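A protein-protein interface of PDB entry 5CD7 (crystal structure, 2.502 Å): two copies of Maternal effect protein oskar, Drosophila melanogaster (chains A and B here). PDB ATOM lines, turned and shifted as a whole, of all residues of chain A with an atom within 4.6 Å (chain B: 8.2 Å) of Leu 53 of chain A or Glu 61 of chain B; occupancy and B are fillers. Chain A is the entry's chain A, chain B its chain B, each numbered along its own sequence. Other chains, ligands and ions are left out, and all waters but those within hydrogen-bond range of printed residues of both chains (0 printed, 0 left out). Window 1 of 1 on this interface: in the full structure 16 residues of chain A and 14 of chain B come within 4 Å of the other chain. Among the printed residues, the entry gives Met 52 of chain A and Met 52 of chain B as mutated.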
ATOM      1  N   THR A  49      25.995 -32.990   7.474  1.00  0.00           N
ATOM      2  CA  THR A  49      25.419 -31.644   7.516  1.00  0.00           C
ATOM      3  C   THR A  49      25.004 -31.336   8.947  1.00  0.00           C
ATOM      4  O   THR A  49      25.280 -30.260   9.481  1.00  0.00           O
ATOM      5  CB  THR A  49      24.209 -31.484   6.557  1.00  0.00           C
ATOM      6  OG1 THR A  49      24.648 -31.561   5.192  1.00  0.00           O
ATOM      7  CG2 THR A  49      23.524 -30.145   6.782  1.00  0.00           C
ATOM      8  N   ASP A  50      24.355 -32.303   9.577  1.00  0.00           N
ATOM      9  CA  ASP A  50      23.944 -32.163  10.966  1.00  0.00           C
ATOM     10  C   ASP A  50      25.160 -31.930  11.872  1.00  0.00           C
ATOM     11  O   ASP A  50      25.116 -31.131  12.820  1.00  0.00           O
ATOM     12  CB  ASP A  50      23.196 -33.414  11.396  1.00  0.00           C
ATOM     13  CG  ASP A  50      22.351 -33.188  12.619  1.00  0.00           C
ATOM     14  OD1 ASP A  50      21.150 -33.523  12.575  1.00  0.00           O
ATOM     15  OD2 ASP A  50      22.885 -32.675  13.622  1.00  0.00           O
ATOM     16  N   PHE A  51      26.255 -32.620  11.576  1.00  0.00           N
ATOM     17  CA  PHE A  51      27.445 -32.449  12.387  1.00  0.00           C
ATOM     18  C   PHE A  51      28.023 -31.038  12.234  1.00  0.00           C
ATOM     19  O   PHE A  51      28.318 -30.368  13.222  1.00  0.00           O
ATOM     20  CB  PHE A  51      28.496 -33.499  12.052  1.00  0.00           C
ATOM     21  CG  PHE A  51      29.782 -33.278  12.757  1.00  0.00           C
ATOM     22  CD1 PHE A  51      29.984 -33.790  14.022  1.00  0.00           C
ATOM     23  CD2 PHE A  51      30.777 -32.519  12.176  1.00  0.00           C
ATOM     24  CE1 PHE A  51      31.172 -33.569  14.682  1.00  0.00           C
ATOM     25  CE2 PHE A  51      31.964 -32.294  12.837  1.00  0.00           C
ATOM     26  CZ  PHE A  51      32.161 -32.817  14.087  1.00  0.00           C
ATOM     27  N   MET A  52      28.185 -30.598  10.991  1.00  0.00           N
ATOM     28  CA  MET A  52      28.618 -29.239  10.693  1.00  0.00           C
ATOM     29  C   MET A  52      27.774 -28.200  11.420  1.00  0.00           C
ATOM     30  O   MET A  52      28.308 -27.259  12.005  1.00  0.00           O
ATOM     31  CB  MET A  52      28.553 -28.993   9.188  1.00  0.00           C
ATOM     32  CG  MET A  52      29.381 -29.973   8.382  1.00  0.00           C
ATOM     33  SD  MET A  52      31.268 -29.901   8.951  1.00  0.00           S
ATOM     34  CE  MET A  52      31.548 -27.993   8.665  1.00  0.00           C
ATOM     35  N   LEU A  53      26.453 -28.382  11.393  1.00  0.00           N
ATOM     36  CA  LEU A  53      25.544 -27.421  12.003  1.00  0.00           C
ATOM     37  C   LEU A  53      25.338 -27.646  13.493  1.00  0.00           C
ATOM     38  O   LEU A  53      24.496 -26.983  14.116  1.00  0.00           O
ATOM     39  CB  LEU A  53      24.199 -27.375  11.267  1.00  0.00           C
ATOM     40  CG  LEU A  53      24.289 -26.533   9.995  1.00  0.00           C
ATOM     41  CD1 LEU A  53      23.201 -26.916   9.030  1.00  0.00           C
ATOM     42  CD2 LEU A  53      24.245 -25.048  10.333  1.00  0.00           C
ATOM     43  N   THR A  54      26.065 -28.604  14.062  1.00  0.00           N
ATOM     44  CA  THR A  54      26.153 -28.653  15.521  1.00  0.00           C
ATOM     45  C   THR A  54      27.271 -27.728  16.046  1.00  0.00           C
ATOM     46  O   THR A  54      27.402 -27.506  17.253  1.00  0.00           O
ATOM     47  CB  THR A  54      26.285 -30.092  16.059  1.00  0.00           C
ATOM     48  OG1 THR A  54      25.263 -30.916  15.475  1.00  0.00           O
ATOM     49  CG2 THR A  54      26.107 -30.105  17.570  1.00  0.00           C
ATOM     50  N   ILE A  55      28.047 -27.160  15.127  1.00  0.00           N
ATOM     51  CA  ILE A  55      29.153 -26.280  15.486  1.00  0.00           C
ATOM     52  C   ILE A  55      28.752 -24.807  15.419  1.00  0.00           C
ATOM     53  O   ILE A  55      28.318 -24.328  14.370  1.00  0.00           O
ATOM     54  CB  ILE A  55      30.353 -26.470  14.535  1.00  0.00           C
ATOM     55  CG1 ILE A  55      30.745 -27.942  14.423  1.00  0.00           C
ATOM     56  CG2 ILE A  55      31.537 -25.613  14.980  1.00  0.00           C
ATOM     57  CD1 ILE A  55      31.768 -28.174  13.323  1.00  0.00           C
ATOM     58  N   VAL A  58      28.385 -21.325  12.570  1.00  0.00           N
ATOM     59  CA  VAL A  58      28.420 -21.919  11.231  1.00  0.00           C
ATOM     60  C   VAL A  58      27.121 -21.660  10.455  1.00  0.00           C
ATOM     61  O   VAL A  58      26.026 -21.736  11.008  1.00  0.00           O
ATOM     62  CB  VAL A  58      28.699 -23.439  11.302  1.00  0.00           C
ATOM     63  CG1 VAL A  58      28.618 -24.079   9.919  1.00  0.00           C
ATOM     64  CG2 VAL A  58      30.075 -23.693  11.929  1.00  0.00           C
ATOM     65  N   THR A  59      27.253 -21.309   9.179  1.00  0.00           N
ATOM     66  CA  THR A  59      26.103 -21.156   8.299  1.00  0.00           C
ATOM     67  C   THR A  59      26.294 -22.063   7.108  1.00  0.00           C
ATOM     68  O   THR A  59      27.424 -22.388   6.735  1.00  0.00           O
ATOM     69  CB  THR A  59      25.948 -19.736   7.753  1.00  0.00           C
ATOM     70  OG1 THR A  59      27.118 -19.385   7.005  1.00  0.00           O
ATOM     71  CG2 THR A  59      25.738 -18.742   8.870  1.00  0.00           C
ATOM     72  N   ALA A  60      25.180 -22.451   6.503  1.00  0.00           N
ATOM     73  CA  ALA A  60      25.197 -23.350   5.365  1.00  0.00           C
ATOM     74  C   ALA A  60      24.122 -22.944   4.371  1.00  0.00           C
ATOM     75  O   ALA A  60      23.122 -22.303   4.736  1.00  0.00           O
ATOM     76  CB  ALA A  60      24.976 -24.774   5.826  1.00  0.00           C
ATOM     77  N   LYS A  73      30.224 -17.670  10.563  1.00  0.00           N
ATOM     78  CA  LYS A  73      29.477 -16.423  10.606  1.00  0.00           C
ATOM     79  C   LYS A  73      30.396 -15.241  10.885  1.00  0.00           C
ATOM     80  O   LYS A  73      31.269 -15.308  11.749  1.00  0.00           O
ATOM     81  CB  LYS A  73      28.385 -16.476  11.676  1.00  0.00           C
ATOM     82  CG  LYS A  73      27.049 -16.983  11.188  1.00  0.00           C
ATOM     83  CD  LYS A  73      25.988 -16.832  12.268  1.00  0.00           C
ATOM     84  CE  LYS A  73      25.792 -15.368  12.653  1.00  0.00           C
ATOM     85  NZ  LYS A  73      24.999 -15.216  13.900  1.00  0.00           N
ATOM     86  N   GLY B  24      13.164 -16.155  11.311  1.00  0.00           N
ATOM     87  CA  GLY B  24      13.987 -17.339  11.469  1.00  0.00           C
ATOM     88  C   GLY B  24      13.162 -18.374  12.201  1.00  0.00           C
ATOM     89  O   GLY B  24      12.272 -18.027  12.977  1.00  0.00           O
ATOM     90  N   ILE B  25      13.425 -19.650  11.964  1.00  0.00           N
ATOM     91  CA  ILE B  25      12.585 -20.658  12.580  1.00  0.00           C
ATOM     92  C   ILE B  25      13.398 -21.873  12.995  1.00  0.00           C
ATOM     93  O   ILE B  25      14.218 -22.369  12.234  1.00  0.00           O
ATOM     94  CB  ILE B  25      11.407 -21.068  11.635  1.00  0.00           C
ATOM     95  CG1 ILE B  25      10.246 -21.665  12.434  1.00  0.00           C
ATOM     96  CG2 ILE B  25      11.878 -22.022  10.545  1.00  0.00           C
ATOM     97  CD1 ILE B  25       9.122 -22.217  11.570  1.00  0.00           C
ATOM     98  N   THR B  26      13.164 -22.354  14.207  1.00  0.00           N
ATOM     99  CA  THR B  26      13.859 -23.537  14.669  1.00  0.00           C
ATOM    100  C   THR B  26      13.189 -24.785  14.129  1.00  0.00           C
ATOM    101  O   THR B  26      12.162 -24.717  13.455  1.00  0.00           O
ATOM    102  CB  THR B  26      13.868 -23.621  16.189  1.00  0.00           C
ATOM    103  OG1 THR B  26      12.521 -23.744  16.663  1.00  0.00           O
ATOM    104  CG2 THR B  26      14.510 -22.374  16.782  1.00  0.00           C
ATOM    105  N   ILE B  27      13.776 -25.934  14.436  1.00  0.00           N
ATOM    106  CA  ILE B  27      13.199 -27.198  14.020  1.00  0.00           C
ATOM    107  C   ILE B  27      11.864 -27.442  14.721  1.00  0.00           C
ATOM    108  O   ILE B  27      10.842 -27.631  14.072  1.00  0.00           O
ATOM    109  CB  ILE B  27      14.157 -28.356  14.308  1.00  0.00           C
ATOM    110  CG1 ILE B  27      15.369 -28.270  13.374  1.00  0.00           C
ATOM    111  CG2 ILE B  27      13.428 -29.690  14.156  1.00  0.00           C
ATOM    112  CD1 ILE B  27      16.620 -28.943  13.912  1.00  0.00           C
ATOM    113  N   VAL B  48      16.673 -33.552  10.058  1.00  0.00           N
ATOM    114  CA  VAL B  48      15.751 -32.624   9.424  1.00  0.00           C
ATOM    115  C   VAL B  48      16.537 -31.512   8.752  1.00  0.00           C
ATOM    116  O   VAL B  48      16.078 -30.909   7.781  1.00  0.00           O
ATOM    117  CB  VAL B  48      14.759 -32.002  10.434  1.00  0.00           C
ATOM    118  CG1 VAL B  48      13.724 -31.155   9.704  1.00  0.00           C
ATOM    119  CG2 VAL B  48      14.075 -33.088  11.247  1.00  0.00           C
ATOM    120  N   THR B  49      17.731 -31.244   9.269  1.00  0.00           N
ATOM    121  CA  THR B  49      18.563 -30.192   8.702  1.00  0.00           C
ATOM    122  C   THR B  49      18.890 -30.506   7.239  1.00  0.00           C
ATOM    123  O   THR B  49      18.810 -29.632   6.369  1.00  0.00           O
ATOM    124  CB  THR B  49      19.852 -29.952   9.536  1.00  0.00           C
ATOM    125  OG1 THR B  49      19.530 -29.930  10.935  1.00  0.00           O
ATOM    126  CG2 THR B  49      20.469 -28.624   9.169  1.00  0.00           C
ATOM    127  N   ASP B  50      19.228 -31.762   6.965  1.00  0.00           N
ATOM    128  CA  ASP B  50      19.526 -32.186   5.602  1.00  0.00           C
ATOM    129  C   ASP B  50      18.326 -31.941   4.671  1.00  0.00           C
ATOM    130  O   ASP B  50      18.462 -31.349   3.582  1.00  0.00           O
ATOM    131  CB  ASP B  50      19.941 -33.658   5.594  1.00  0.00           C
ATOM    132  CG  ASP B  50      20.348 -34.147   4.220  1.00  0.00           C
ATOM    133  OD1 ASP B  50      21.408 -33.721   3.716  1.00  0.00           O
ATOM    134  OD2 ASP B  50      19.622 -34.983   3.646  1.00  0.00           O
ATOM    135  N   MET B  52      15.713 -29.900   5.104  1.00  0.00           N
ATOM    136  CA  MET B  52      15.541 -28.467   4.949  1.00  0.00           C
ATOM    137  C   MET B  52      16.501 -27.897   3.921  1.00  0.00           C
ATOM    138  O   MET B  52      16.112 -27.066   3.091  1.00  0.00           O
ATOM    139  CB  MET B  52      15.765 -27.751   6.270  1.00  0.00           C
ATOM    140  CG  MET B  52      14.831 -28.178   7.366  1.00  0.00           C
ATOM    141  SD  MET B  52      12.958 -27.866   6.901  1.00  0.00           S
ATOM    142  CE  MET B  52      13.006 -25.962   6.459  1.00  0.00           C
ATOM    143  N   LEU B  53      17.766 -28.321   3.984  1.00  0.00           N
ATOM    144  CA  LEU B  53      18.759 -27.778   3.068  1.00  0.00           C
ATOM    145  C   LEU B  53      18.519 -28.211   1.634  1.00  0.00           C
ATOM    146  O   LEU B  53      18.951 -27.521   0.707  1.00  0.00           O
ATOM    147  CB  LEU B  53      20.189 -28.115   3.502  1.00  0.00           C
ATOM    148  CG  LEU B  53      20.690 -27.262   4.670  1.00  0.00           C
ATOM    149  CD1 LEU B  53      22.170 -27.486   4.896  1.00  0.00           C
ATOM    150  CD2 LEU B  53      20.397 -25.792   4.410  1.00  0.00           C
ATOM    151  N   VAL B  58      16.859 -21.881   0.885  1.00  0.00           N
ATOM    152  CA  VAL B  58      16.868 -21.979   2.343  1.00  0.00           C
ATOM    153  C   VAL B  58      18.284 -21.951   2.908  1.00  0.00           C
ATOM    154  O   VAL B  58      19.196 -22.533   2.330  1.00  0.00           O
ATOM    155  CB  VAL B  58      16.143 -23.247   2.842  1.00  0.00           C
ATOM    156  CG1 VAL B  58      16.208 -23.343   4.368  1.00  0.00           C
ATOM    157  CG2 VAL B  58      14.691 -23.241   2.370  1.00  0.00           C
ATOM    158  N   THR B  59      18.459 -21.252   4.028  1.00  0.00           N
ATOM    159  CA  THR B  59      19.733 -21.228   4.715  1.00  0.00           C
ATOM    160  C   THR B  59      19.575 -21.732   6.136  1.00  0.00           C
ATOM    161  O   THR B  59      18.546 -21.492   6.776  1.00  0.00           O
ATOM    162  CB  THR B  59      20.333 -19.810   4.798  1.00  0.00           C
ATOM    163  OG1 THR B  59      19.568 -19.014   5.713  1.00  0.00           O
ATOM    164  CG2 THR B  59      20.364 -19.152   3.434  1.00  0.00           C
ATOM    165  N   ALA B  60      20.622 -22.398   6.626  1.00  0.00           N
ATOM    166  CA  ALA B  60      20.659 -22.895   7.992  1.00  0.00           C
ATOM    167  C   ALA B  60      21.742 -22.164   8.743  1.00  0.00           C
ATOM    168  O   ALA B  60      22.695 -21.669   8.152  1.00  0.00           O
ATOM    169  CB  ALA B  60      20.945 -24.375   8.011  1.00  0.00           C
ATOM    170  N   GLU B  61      21.596 -22.087  10.054  1.00  0.00           N
ATOM    171  CA  GLU B  61      22.626 -21.482  10.859  1.00  0.00           C
ATOM    172  C   GLU B  61      22.691 -22.101  12.250  1.00  0.00           C
ATOM    173  O   GLU B  61      21.670 -22.354  12.875  1.00  0.00           O
ATOM    174  CB  GLU B  61      22.372 -19.982  10.941  1.00  0.00           C
ATOM    175  CG  GLU B  61      22.991 -19.291  12.132  1.00  0.00           C
ATOM    176  CD  GLU B  61      22.484 -17.873  12.281  1.00  0.00           C
ATOM    177  OE1 GLU B  61      22.899 -17.182  13.237  1.00  0.00           O
ATOM    178  OE2 GLU B  61      21.659 -17.460  11.433  1.00  0.00           O
ATOM    179  N   CYS B  62      23.903 -22.333  12.741  1.00  0.00           N
ATOM    180  CA  CYS B  62      24.083 -22.654  14.148  1.00  0.00           C
ATOM    181  C   CYS B  62      24.640 -21.387  14.773  1.00  0.00           C
ATOM    182  O   CYS B  62      25.674 -20.898  14.343  1.00  0.00           O
ATOM    183  CB  CYS B  62      25.031 -23.834  14.324  1.00  0.00           C
ATOM    184  SG  CYS B  62      25.092 -24.490  16.003  1.00  0.00           S
ATOM    185  N   SER B  63      23.934 -20.828  15.749  1.00  0.00           N
ATOM    186  CA  SER B  63      24.274 -19.503  16.257  1.00  0.00           C
ATOM    187  C   SER B  63      25.488 -19.562  17.179  1.00  0.00           C
ATOM    188  O   SER B  63      26.060 -20.631  17.391  1.00  0.00           O
ATOM    189  CB  SER B  63      23.076 -18.870  16.979  1.00  0.00           C
ATOM    190  OG  SER B  63      22.830 -19.488  18.233  1.00  0.00           O
ATOM    191  N   GLU B  64      25.886 -18.412  17.715  1.00  0.00           N
ATOM    192  CA  GLU B  64      26.980 -18.369  18.677  1.00  0.00           C
ATOM    193  C   GLU B  64      26.650 -19.245  19.881  1.00  0.00           C
ATOM    194  O   GLU B  64      27.533 -19.871  20.470  1.00  0.00           O
ATOM    195  CB  GLU B  64      27.249 -16.932  19.134  1.00  0.00           C
ATOM    196  CG  GLU B  64      28.172 -16.128  18.227  1.00  0.00           C
ATOM    197  CD  GLU B  64      27.471 -15.550  17.009  1.00  0.00           C
ATOM    198  OE1 GLU B  64      26.341 -15.989  16.691  1.00  0.00           O
ATOM    199  OE2 GLU B  64      28.056 -14.646  16.371  1.00  0.00           O
ATOM    200  N   SER B  65      25.369 -19.281  20.237  1.00  0.00           N
ATOM    201  CA  SER B  65      24.908 -20.030  21.405  1.00  0.00           C
ATOM    202  C   SER B  65      24.370 -21.435  21.106  1.00  0.00           C
ATOM    203  O   SER B  65      23.880 -22.115  22.006  1.00  0.00           O
ATOM    204  CB  SER B  65      23.877 -19.215  22.190  1.00  0.00           C
ATOM    205  OG  SER B  65      24.498 -18.121  22.847  1.00  0.00           O
ATOM    206  N   GLY B  66      24.444 -21.860  19.848  1.00  0.00           N
ATOM    207  CA  GLY B  66      24.103 -23.227  19.494  1.00  0.00           C
ATOM    208  C   GLY B  66      22.661 -23.405  19.057  1.00  0.00           C
ATOM    209  O   GLY B  66      22.157 -24.528  18.981  1.00  0.00           O
ATOM    210  N   LYS B  67      21.996 -22.294  18.763  1.00  0.00           N
ATOM    211  CA  LYS B  67      20.618 -22.327  18.303  1.00  0.00           C
ATOM    212  C   LYS B  67      20.572 -22.602  16.808  1.00  0.00           C
ATOM    213  O   LYS B  67      21.125 -21.841  16.014  1.00  0.00           O
ATOM    214  CB  LYS B  67      19.942 -20.994  18.610  1.00  0.00           C
ATOM    215  CG  LYS B  67      18.424 -21.015  18.549  1.00  0.00           C
ATOM    216  CD  LYS B  67      17.876 -19.736  19.165  1.00  0.00           C
ATOM    217  CE  LYS B  67      16.364 -19.688  19.150  1.00  0.00           C
ATOM    218  NZ  LYS B  67      15.876 -18.503  19.911  1.00  0.00           N
ATOM    219  N   ARG B  68      19.909 -23.689  16.425  1.00  0.00           N
ATOM    220  CA  ARG B  68      19.774 -24.055  15.023  1.00  0.00           C
ATOM    221  C   ARG B  68      18.579 -23.313  14.413  1.00  0.00           C
ATOM    222  O   ARG B  68      17.431 -23.526  14.817  1.00  0.00           O
ATOM    223  CB  ARG B  68      19.528 -25.558  14.915  1.00  0.00           C
ATOM    224  CG  ARG B  68      20.390 -26.304  13.927  1.00  0.00           C
ATOM    225  CD  ARG B  68      21.454 -27.067  14.689  1.00  0.00           C
ATOM    226  NE  ARG B  68      21.888 -28.268  13.984  1.00  0.00           N
ATOM    227  CZ  ARG B  68      21.486 -29.496  14.288  1.00  0.00           C
ATOM    228  NH1 ARG B  68      21.934 -30.531  13.592  1.00  0.00           N
ATOM    229  NH2 ARG B  68      20.641 -29.689  15.294  1.00  0.00           N
ATOM    230  N   ILE B  69      18.834 -22.462  13.427  1.00  0.00           N
ATOM    231  CA  ILE B  69      17.756 -21.667  12.858  1.00  0.00           C
ATOM    232  C   ILE B  69      17.763 -21.672  11.335  1.00  0.00           C
ATOM    233  O   ILE B  69      18.816 -21.579  10.703  1.00  0.00           O
ATOM    234  CB  ILE B  69      17.762 -20.217  13.405  1.00  0.00           C
ATOM    235  CG1 ILE B  69      16.333 -19.713  13.563  1.00  0.00           C
ATOM    236  CG2 ILE B  69      18.559 -19.288  12.505  1.00  0.00           C
ATOM    237  CD1 ILE B  69      16.238 -18.325  14.139  1.00  0.00           C
ATOM    238  N   PHE B  70      16.574 -21.793  10.760  1.00  0.00           N
ATOM    239  CA  PHE B  70      16.402 -21.821   9.309  1.00  0.00           C
ATOM    240  C   PHE B  70      15.663 -20.592   8.788  1.00  0.00           C
ATOM    241  O   PHE B  70      14.803 -20.016   9.467  1.00  0.00           O
ATOM    242  CB  PHE B  70      15.670 -23.091   8.888  1.00  0.00           C
ATOM    243  CG  PHE B  70      16.360 -24.343   9.324  1.00  0.00           C
ATOM    244  CD1 PHE B  70      16.240 -24.796  10.622  1.00  0.00           C
ATOM    245  CD2 PHE B  70      17.149 -25.059   8.440  1.00  0.00           C
ATOM    246  CE1 PHE B  70      16.894 -25.953  11.035  1.00  0.00           C
ATOM    247  CE2 PHE B  70      17.802 -26.214   8.848  1.00  0.00           C
ATOM    248  CZ  PHE B  70      17.665 -26.662  10.149  1.00  0.00           C
ATOM    249  N   ASN B  71      16.009 -20.207   7.567  1.00  0.00           N
ATOM    250  CA  ASN B  71      15.533 -18.967   6.984  1.00  0.00           C
ATOM    251  C   ASN B  71      15.395 -19.112   5.488  1.00  0.00           C
ATOM    252  O   ASN B  71      15.933 -20.051   4.890  1.00  0.00           O
ATOM    253  CB  ASN B  71      16.528 -17.836   7.269  1.00  0.00           C
ATOM    254  CG  ASN B  71      16.275 -17.154   8.593  1.00  0.00           C
ATOM    255  OD1 ASN B  71      15.169 -16.679   8.860  1.00  0.00           O
ATOM    256  ND2 ASN B  71      17.296 -17.101   9.433  1.00  0.00           N
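The guanidinium group of Arg 68 of chain B is in salt-bridge range of the side-chain carboxylate of Asp 50 of chain A (3.3 Å).
SG of Cys 62 of chain B is in hydrogen-bond range of O of Leu 53 of chain A (3.2 Å).
NE of Arg 68 of chain B lies within hydrogen-bond range of O of Leu 53 of chain A (2.9 Å).
The backbone carbonyl oxygen (O) of Ile 55 of chain A sits close to the side-chain sulfur (SG) of Cys 62 of chain B (3.6 Å).
N of Cys 62 of chain B is in hydrogen-bond range of O of Val 58 of chain A (2.8 Å).
N of Ala 60 of chain A lies within hydrogen-bond range of O of Ala 60 of chain B.
OE1 of Glu 61 of chain B lies within salt-bridge range of NZ of Lys 73 of chain A, 3.0 Å away.
NZ of Lys 73 of chain A is in salt-bridge range of OE1 of Glu 64 of chain B.
Printed residues of chain A that touch a printed residue of chain B: Thr 49, Asp 50, Leu 53, Thr 54, Ile 55, Val 58, Thr 59, Ala 60 and Lys 73.
Along chain A the printed residues that touch a printed residue of chain B span positions 49 to 73.
Printed residues of chain B that touch a printed residue of chain A: Thr 49, Leu 53, Thr 59, Ala 60, Glu 61, Cys 62, Glu 64 and Arg 68.
Among the printed residues, 17 pairs touch across the chains.
Thr 49 of chain A touches Leu 53 of chain B, and with the chains exchanged Leu 53 of chain A touches Thr 49 of chain B.
Leu 53 of chain A touches Ala 60 of chain B, but with the chains exchanged Ala 60 of chain A does not touch Leu 53 of chain B (4.01 Å).
Thr 59 of chain A touches Ala 60 of chain B, and with the chains exchanged Ala 60 of chain A touches Thr 59 of chain B.
Ala 60 of chain B touches its own counterpart, Ala 60 of chain A.
Positions printed for both chains: 49, 50, 52, 53, 58, 59 and 60.
Of the 17 pairs that touch across the chains among the printed residues, 5 have their exchanged pair printed and touching as well.
Of chain B, only Thr 49 (3.2 Å), Ala 60 (3.5 Å), Glu 61 (3.8 Å), Cys 62 (3.2 Å) and Arg 68 (2.9 Å) come within 4 Å of Leu 53 of chain A.
Printed residues of chain B within 4 Å of Ile 55 of chain A: Cys 62.
Of the printed residues of chain A, Leu 53 of chain B touches Thr 49 (3.5 Å).
Of the printed residues of chain B, Asp 50 of chain A touches Arg 68 (2.3 Å).
Printed residues of chain B within 4 Å of Ala 60 of chain A: Thr 59 and Ala 60.
Lys 67 of chain B touches none of the printed residues of chain A.
Ile 25 of chain B touches none of the printed residues of chain A.
The nearest residue of chain B that does not touch Leu 53 of chain A is Leu 53 of chain B (4.3 Å).
The nearest printed residue of chain A that does not touch Thr 59 of chain B is Thr 59 of chain A (6.3 Å).
Among the printed residues, merely in contact across the chains: Thr 49 of chain A with Leu 53 of chain B (3.5 Å), Leu 53 of chain A with Thr 49 of chain B (3.2 Å), Leu 53 of chain A with Ala 60 of chain B (3.5 Å), Leu 53 of chain A with Glu 61 of chain B (3.8 Å), Thr 54 of chain A with Cys 62 of chain B (3.9 Å), Thr 54 of chain A with Arg 68 of chain B (3.8 Å), Val 58 of chain A with Glu 61 of chain B (3.4 Å), Thr 59 of chain A with Ala 60 of chain B (3.4 Å) and Ala 60 of chain A with Thr 59 of chain B (3.6 Å).
The side-chain hydroxyl (OG1) of Thr 54 of chain A is in hydrogen-bond range of the backbone carbonyl oxygen (O) of Asp 50 of chain A (2.7 Å).
N of Thr 59 of chain B lies within hydrogen-bond range of O of Asn 71 of chain B (2.9 Å).
The backbone carbonyl oxygen of Glu 61 of chain B lies within hydrogen-bond range of the backbone NH of Ile 69 of chain B (2.9 Å).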
